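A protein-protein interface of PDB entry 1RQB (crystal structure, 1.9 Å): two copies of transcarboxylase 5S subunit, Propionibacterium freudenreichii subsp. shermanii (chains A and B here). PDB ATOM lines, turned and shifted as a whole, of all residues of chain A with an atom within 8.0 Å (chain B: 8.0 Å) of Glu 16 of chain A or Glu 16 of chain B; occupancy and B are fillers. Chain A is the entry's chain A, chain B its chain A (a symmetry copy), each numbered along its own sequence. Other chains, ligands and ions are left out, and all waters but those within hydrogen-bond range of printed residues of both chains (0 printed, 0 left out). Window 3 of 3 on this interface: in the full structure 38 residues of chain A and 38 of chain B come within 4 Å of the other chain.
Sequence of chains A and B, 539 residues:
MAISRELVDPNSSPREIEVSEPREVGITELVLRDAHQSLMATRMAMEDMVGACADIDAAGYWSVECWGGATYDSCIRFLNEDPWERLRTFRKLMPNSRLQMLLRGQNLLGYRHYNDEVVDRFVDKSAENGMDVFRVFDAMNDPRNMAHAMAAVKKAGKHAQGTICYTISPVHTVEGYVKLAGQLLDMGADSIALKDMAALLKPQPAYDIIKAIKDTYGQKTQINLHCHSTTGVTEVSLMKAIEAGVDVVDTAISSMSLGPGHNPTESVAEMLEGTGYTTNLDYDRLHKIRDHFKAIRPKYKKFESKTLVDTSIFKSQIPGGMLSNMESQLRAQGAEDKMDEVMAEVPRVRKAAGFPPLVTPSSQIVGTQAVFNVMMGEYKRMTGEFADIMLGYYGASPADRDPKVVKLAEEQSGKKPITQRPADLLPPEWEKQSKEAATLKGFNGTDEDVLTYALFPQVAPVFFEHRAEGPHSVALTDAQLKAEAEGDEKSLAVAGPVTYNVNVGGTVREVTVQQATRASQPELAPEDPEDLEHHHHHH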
ATOM      1  N   PRO A  14     -27.613  20.762  -2.047  1.00  0.00           N
ATOM      2  CA  PRO A  14     -28.108  21.461  -3.254  1.00  0.00           C
ATOM      3  C   PRO A  14     -28.468  22.923  -2.988  1.00  0.00           C
ATOM      4  O   PRO A  14     -29.121  23.266  -2.002  1.00  0.00           O
ATOM      5  CB  PRO A  14     -29.309  20.679  -3.755  1.00  0.00           C
ATOM      6  CG  PRO A  14     -28.934  19.273  -3.306  1.00  0.00           C
ATOM      7  CD  PRO A  14     -28.301  19.465  -1.909  1.00  0.00           C
ATOM      8  N   ARG A  15     -28.027  23.765  -3.905  1.00  0.00           N
ATOM      9  CA  ARG A  15     -28.223  25.221  -3.857  1.00  0.00           C
ATOM     10  C   ARG A  15     -28.888  25.664  -5.160  1.00  0.00           C
ATOM     11  O   ARG A  15     -29.159  24.845  -6.037  1.00  0.00           O
ATOM     12  CB  ARG A  15     -26.837  25.836  -3.640  1.00  0.00           C
ATOM     13  CG  ARG A  15     -25.794  25.071  -4.430  1.00  0.00           C
ATOM     14  CD  ARG A  15     -24.396  25.124  -3.830  1.00  0.00           C
ATOM     15  NE  ARG A  15     -23.683  26.379  -3.987  1.00  0.00           N
ATOM     16  CZ  ARG A  15     -22.721  26.561  -4.887  1.00  0.00           C
ATOM     17  NH1 ARG A  15     -22.378  25.569  -5.699  1.00  0.00           N
ATOM     18  NH2 ARG A  15     -22.079  27.719  -4.953  1.00  0.00           N
ATOM     19  N   GLU A  16     -29.180  26.946  -5.287  1.00  0.00           N
ATOM     20  CA  GLU A  16     -29.835  27.409  -6.518  1.00  0.00           C
ATOM     21  C   GLU A  16     -29.214  28.728  -6.982  1.00  0.00           C
ATOM     22  O   GLU A  16     -28.689  29.505  -6.186  1.00  0.00           O
ATOM     23  CB  GLU A  16     -31.319  27.626  -6.279  1.00  0.00           C
ATOM     24  CG  GLU A  16     -32.025  26.418  -5.724  1.00  0.00           C
ATOM     25  CD  GLU A  16     -33.489  26.411  -6.079  1.00  0.00           C
ATOM     26  OE1 GLU A  16     -33.843  25.791  -7.108  1.00  0.00           O
ATOM     27  OE2 GLU A  16     -34.281  27.037  -5.340  1.00  0.00           O
ATOM     28  N   ILE A  17     -29.278  28.950  -8.286  1.00  0.00           N
ATOM     29  CA  ILE A  17     -28.773  30.198  -8.874  1.00  0.00           C
ATOM     30  C   ILE A  17     -29.903  30.855  -9.668  1.00  0.00           C
ATOM     31  O   ILE A  17     -30.567  30.210 -10.479  1.00  0.00           O
ATOM     32  CB  ILE A  17     -27.606  29.940  -9.836  1.00  0.00           C
ATOM     33  CG1 ILE A  17     -26.411  29.389  -9.067  1.00  0.00           C
ATOM     34  CG2 ILE A  17     -27.225  31.244 -10.537  1.00  0.00           C
ATOM     35  CD1 ILE A  17     -25.291  28.896  -9.960  1.00  0.00           C
ATOM     36  N   GLU A  18     -30.133  32.133  -9.416  1.00  0.00           N
ATOM     37  CA  GLU A  18     -31.176  32.864 -10.145  1.00  0.00           C
ATOM     38  C   GLU A  18     -30.649  33.184 -11.545  1.00  0.00           C
ATOM     39  O   GLU A  18     -29.518  33.646 -11.692  1.00  0.00           O
ATOM     40  CB  GLU A  18     -31.502  34.150  -9.398  1.00  0.00           C
ATOM     41  CG  GLU A  18     -32.540  35.021 -10.070  1.00  0.00           C
ATOM     42  CD  GLU A  18     -32.987  36.146  -9.165  1.00  0.00           C
ATOM     43  OE1 GLU A  18     -33.704  35.858  -8.181  1.00  0.00           O
ATOM     44  OE2 GLU A  18     -32.610  37.310  -9.424  1.00  0.00           O
ATOM     45  N   VAL A  19     -31.452  32.922 -12.574  1.00  0.00           N
ATOM     46  CA  VAL A  19     -31.017  33.216 -13.947  1.00  0.00           C
ATOM     47  C   VAL A  19     -32.089  34.065 -14.632  1.00  0.00           C
ATOM     48  O   VAL A  19     -33.257  34.034 -14.245  1.00  0.00           O
ATOM     49  CB  VAL A  19     -30.742  31.925 -14.761  1.00  0.00           C
ATOM     50  CG1 VAL A  19     -29.621  31.135 -14.093  1.00  0.00           C
ATOM     51  CG2 VAL A  19     -32.008  31.068 -14.871  1.00  0.00           C
ATOM     52  N   SER A  20     -31.690  34.819 -15.648  1.00  0.00           N
ATOM     53  CA  SER A  20     -32.630  35.715 -16.336  1.00  0.00           C
ATOM     54  C   SER A  20     -33.702  34.922 -17.083  1.00  0.00           C
ATOM     55  O   SER A  20     -33.550  33.736 -17.377  1.00  0.00           O
ATOM     56  CB  SER A  20     -31.881  36.653 -17.298  1.00  0.00           C
ATOM     57  OG  SER A  20     -31.100  35.930 -18.237  1.00  0.00           O
ATOM     58  N   TYR A 207     -20.975  37.155 -13.731  1.00  0.00           N
ATOM     59  CA  TYR A 207     -22.352  37.075 -13.221  1.00  0.00           C
ATOM     60  C   TYR A 207     -22.596  38.159 -12.166  1.00  0.00           C
ATOM     61  O   TYR A 207     -23.558  38.920 -12.256  1.00  0.00           O
ATOM     62  CB  TYR A 207     -22.587  35.687 -12.604  1.00  0.00           C
ATOM     63  CG  TYR A 207     -23.972  35.505 -12.018  1.00  0.00           C
ATOM     64  CD1 TYR A 207     -25.011  34.959 -12.780  1.00  0.00           C
ATOM     65  CD2 TYR A 207     -24.249  35.894 -10.709  1.00  0.00           C
ATOM     66  CE1 TYR A 207     -26.294  34.810 -12.240  1.00  0.00           C
ATOM     67  CE2 TYR A 207     -25.528  35.745 -10.161  1.00  0.00           C
ATOM     68  CZ  TYR A 207     -26.541  35.206 -10.929  1.00  0.00           C
ATOM     69  OH  TYR A 207     -27.798  35.064 -10.390  1.00  0.00           O
ATOM     70  N   PRO B  14     -37.694  36.095 -13.780  1.00  0.00           N
ATOM     71  CA  PRO B  14     -36.571  35.375 -13.142  1.00  0.00           C
ATOM     72  C   PRO B  14     -36.925  33.936 -12.761  1.00  0.00           C
ATOM     73  O   PRO B  14     -37.983  33.651 -12.202  1.00  0.00           O
ATOM     74  CB  PRO B  14     -36.164  36.183 -11.922  1.00  0.00           C
ATOM     75  CG  PRO B  14     -36.522  37.588 -12.387  1.00  0.00           C
ATOM     76  CD  PRO B  14     -37.853  37.419 -13.153  1.00  0.00           C
ATOM     77  N   ARG B  15     -36.000  33.048 -13.079  1.00  0.00           N
ATOM     78  CA  ARG B  15     -36.121  31.603 -12.840  1.00  0.00           C
ATOM     79  C   ARG B  15     -34.909  31.142 -12.031  1.00  0.00           C
ATOM     80  O   ARG B  15     -34.034  31.941 -11.699  1.00  0.00           O
ATOM     81  CB  ARG B  15     -36.219  30.945 -14.220  1.00  0.00           C
ATOM     82  CG  ARG B  15     -35.301  31.644 -15.202  1.00  0.00           C
ATOM     83  CD  ARG B  15     -35.758  31.560 -16.651  1.00  0.00           C
ATOM     84  NE  ARG B  15     -35.575  30.274 -17.301  1.00  0.00           N
ATOM     85  CZ  ARG B  15     -34.591  30.028 -18.160  1.00  0.00           C
ATOM     86  NH1 ARG B  15     -33.712  30.979 -18.451  1.00  0.00           N
ATOM     87  NH2 ARG B  15     -34.502  28.846 -18.753  1.00  0.00           N
ATOM     88  N   GLU B  16     -34.860  29.868 -11.685  1.00  0.00           N
ATOM     89  CA  GLU B  16     -33.719  29.388 -10.893  1.00  0.00           C
ATOM     90  C   GLU B  16     -33.244  28.033 -11.418  1.00  0.00           C
ATOM     91  O   GLU B  16     -34.011  27.264 -11.996  1.00  0.00           O
ATOM     92  CB  GLU B  16     -34.115  29.235  -9.435  1.00  0.00           C
ATOM     93  CG  GLU B  16     -34.692  30.485  -8.830  1.00  0.00           C
ATOM     94  CD  GLU B  16     -34.488  30.535  -7.338  1.00  0.00           C
ATOM     95  OE1 GLU B  16     -33.477  31.133  -6.902  1.00  0.00           O
ATOM     96  OE2 GLU B  16     -35.325  29.963  -6.605  1.00  0.00           O
ATOM     97  N   ILE B  17     -31.962  27.770 -11.214  1.00  0.00           N
ATOM     98  CA  ILE B  17     -31.372  26.485 -11.615  1.00  0.00           C
ATOM     99  C   ILE B  17     -30.721  25.845 -10.388  1.00  0.00           C
ATOM    100  O   ILE B  17     -29.958  26.486  -9.667  1.00  0.00           O
ATOM    101  CB  ILE B  17     -30.288  26.669 -12.685  1.00  0.00           C
ATOM    102  CG1 ILE B  17     -30.911  27.200 -13.970  1.00  0.00           C
ATOM    103  CG2 ILE B  17     -29.601  25.329 -12.948  1.00  0.00           C
ATOM    104  CD1 ILE B  17     -29.893  27.622 -15.009  1.00  0.00           C
ATOM    105  N   GLU B  18     -31.042  24.585 -10.143  1.00  0.00           N
ATOM    106  CA  GLU B  18     -30.450  23.869  -9.007  1.00  0.00           C
ATOM    107  C   GLU B  18     -29.016  23.483  -9.377  1.00  0.00           C
ATOM    108  O   GLU B  18     -28.773  22.976 -10.471  1.00  0.00           O
ATOM    109  CB  GLU B  18     -31.272  22.622  -8.716  1.00  0.00           C
ATOM    110  CG  GLU B  18     -30.741  21.768  -7.586  1.00  0.00           C
ATOM    111  CD  GLU B  18     -31.728  20.690  -7.197  1.00  0.00           C
ATOM    112  OE1 GLU B  18     -32.768  21.037  -6.594  1.00  0.00           O
ATOM    113  OE2 GLU B  18     -31.475  19.505  -7.507  1.00  0.00           O
ATOM    114  N   VAL B  19     -28.064  23.740  -8.482  1.00  0.00           N
ATOM    115  CA  VAL B  19     -26.666  23.385  -8.765  1.00  0.00           C
ATOM    116  C   VAL B  19     -26.125  22.554  -7.600  1.00  0.00           C
ATOM    117  O   VAL B  19     -26.627  22.641  -6.480  1.00  0.00           O
ATOM    118  CB  VAL B  19     -25.782  24.637  -8.998  1.00  0.00           C
ATOM    119  CG1 VAL B  19     -26.303  25.408 -10.206  1.00  0.00           C
ATOM    120  CG2 VAL B  19     -25.769  25.536  -7.757  1.00  0.00           C
ATOM    121  N   SER B  20     -25.103  21.752  -7.868  1.00  0.00           N
ATOM    122  CA  SER B  20     -24.546  20.869  -6.834  1.00  0.00           C
ATOM    123  C   SER B  20     -23.883  21.676  -5.717  1.00  0.00           C
ATOM    124  O   SER B  20     -23.531  22.845  -5.878  1.00  0.00           O
ATOM    125  CB  SER B  20     -23.548  19.873  -7.449  1.00  0.00           C
ATOM    126  OG  SER B  20     -22.510  20.535  -8.153  1.00  0.00           O
ATOM    127  N   TYR B 207     -26.011  19.088 -18.639  1.00  0.00           N
ATOM    128  CA  TYR B 207     -26.654  19.235 -17.325  1.00  0.00           C
ATOM    129  C   TYR B 207     -27.769  18.197 -17.155  1.00  0.00           C
ATOM    130  O   TYR B 207     -27.804  17.470 -16.163  1.00  0.00           O
ATOM    131  CB  TYR B 207     -27.241  20.651 -17.200  1.00  0.00           C
ATOM    132  CG  TYR B 207     -27.956  20.904 -15.890  1.00  0.00           C
ATOM    133  CD1 TYR B 207     -27.284  21.461 -14.797  1.00  0.00           C
ATOM    134  CD2 TYR B 207     -29.300  20.569 -15.735  1.00  0.00           C
ATOM    135  CE1 TYR B 207     -27.945  21.676 -13.581  1.00  0.00           C
ATOM    136  CE2 TYR B 207     -29.969  20.783 -14.524  1.00  0.00           C
ATOM    137  CZ  TYR B 207     -29.288  21.333 -13.457  1.00  0.00           C
ATOM    138  OH  TYR B 207     -29.946  21.539 -12.267  1.00  0.00           O
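The backbone NH (N) of Val 19 of chain B is in hydrogen-bond range of the backbone carbonyl oxygen (O) of Arg 15 of chain A, at 2.9 Å.
The guanidinium group of Arg 15 of chain A sits at hydrogen-bond distance from the backbone carbonyl oxygen of Ser 20 of chain B (3.0 Å).
The backbone NH (N) of Ile 17 of chain A sits at hydrogen-bond distance from the backbone carbonyl oxygen (O) of Ile 17 of chain B.
The backbone NH of Val 19 of chain A sits at hydrogen-bond distance from the backbone carbonyl oxygen of Arg 15 of chain B.
NH1 of Arg 15 of chain B is in hydrogen-bond range of O of Ser 20 of chain A (3.0 Å).
The side-chain carboxylate (OE2) of Glu 16 of chain A sits close to the side-chain carboxylate (OE2) of Glu 16 of chain B, 3.4 Å away.
The backbone carbonyl oxygen (O) of Glu 18 of chain A is in hydrogen-bond range of the side-chain hydroxyl (OH) of Tyr 207 of chain A, at 2.6 Å.
The backbone carbonyl oxygen (O) of Glu 18 of chain B lies within hydrogen-bond range of the side-chain hydroxyl (OH) of Tyr 207 of chain B (2.6 Å).
Among the printed residues, merely in contact across the chains: Ile 17 of chain A with Glu 16 of chain B (3.3 Å), Glu 16 of chain A with Ile 17 of chain B (3.3 Å), Glu 18 of chain A with Arg 15 of chain B (3.4 Å), Arg 15 of chain A with Glu 18 of chain B (3.4 Å), Ile 17 of chain A with Val 19 of chain B (3.6 Å), Val 19 of chain A with Ile 17 of chain B (3.6 Å), Pro 14 of chain A with Val 19 of chain B (3.7 Å) and Val 19 of chain A with Pro 14 of chain B (3.7 Å).
Of chain B, only Glu 16 (3.4 Å) and Ile 17 (3.3 Å) come within 4 Å of Glu 16 of chain A.
Printed residues of chain B within 4 Å of Ile 17 of chain A: Glu 16 (3.3 Å), Ile 17 (2.9 Å) and Val 19 (3.6 Å).
Printed residues of chain B within 4 Å of Ser 20 of chain A: Arg 15.
Tyr 207 of chain A touches none of the printed residues of chain B.
Of the printed residues of chain A, Arg 15 of chain B touches Glu 18 (3.4 Å), Val 19 (2.9 Å) and Ser 20 (3.0 Å).
Glu 16 of chain B touches two residues of chain A.
Printed residues of chain A within 4 Å of Ile 17 of chain B: Glu 16 (3.3 Å), Ile 17 (2.9 Å) and Val 19 (3.6 Å).
Tyr 207 of chain B touches none of the printed residues of chain A.
The nearest residue of chain B that does not touch Glu 16 of chain A is Glu 18 of chain B (4.3 Å).
Of the 8 printed residues of chain B, 7 touch a printed residue of chain A.
Printed residues of chain B that touch a printed residue of chain A: Pro 14, Arg 15, Glu 16, Ile 17, Glu 18, Val 19 and Ser 20.
Hydrophobic or aromatic side chains of chain B within 4 Å of the printed part of chain A: Ile 17 and Val 19.
Of the 8 printed residues of chain A, 7 touch a printed residue of chain B.
Hydrophobic or aromatic side chains of chain A that line the printed part of chain B: Ile 17 and Val 19.
Along chain A the printed residues that touch a printed residue of chain B span positions 14 to 20.
Among the printed residues, 14 pairs touch across the chains.
Glu 16 of chain B touches its own counterpart, Glu 16 of chain A.
Glu 16 of chain A touches Ile 17 of chain B, and with the chains exchanged Ile 17 of chain A touches Glu 16 of chain B.
Ile 17 of chain B touches its own counterpart, Ile 17 of chain A.
Ile 17 of chain A touches Val 19 of chain B, and with the chains exchanged Val 19 of chain A touches Ile 17 of chain B.
Positions printed for both chains: 14, 15, 16, 17, 18, 19, 20 and 207.
Of the 14 pairs that touch across the chains among the printed residues, 14 have their exchanged pair printed and touching as well.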
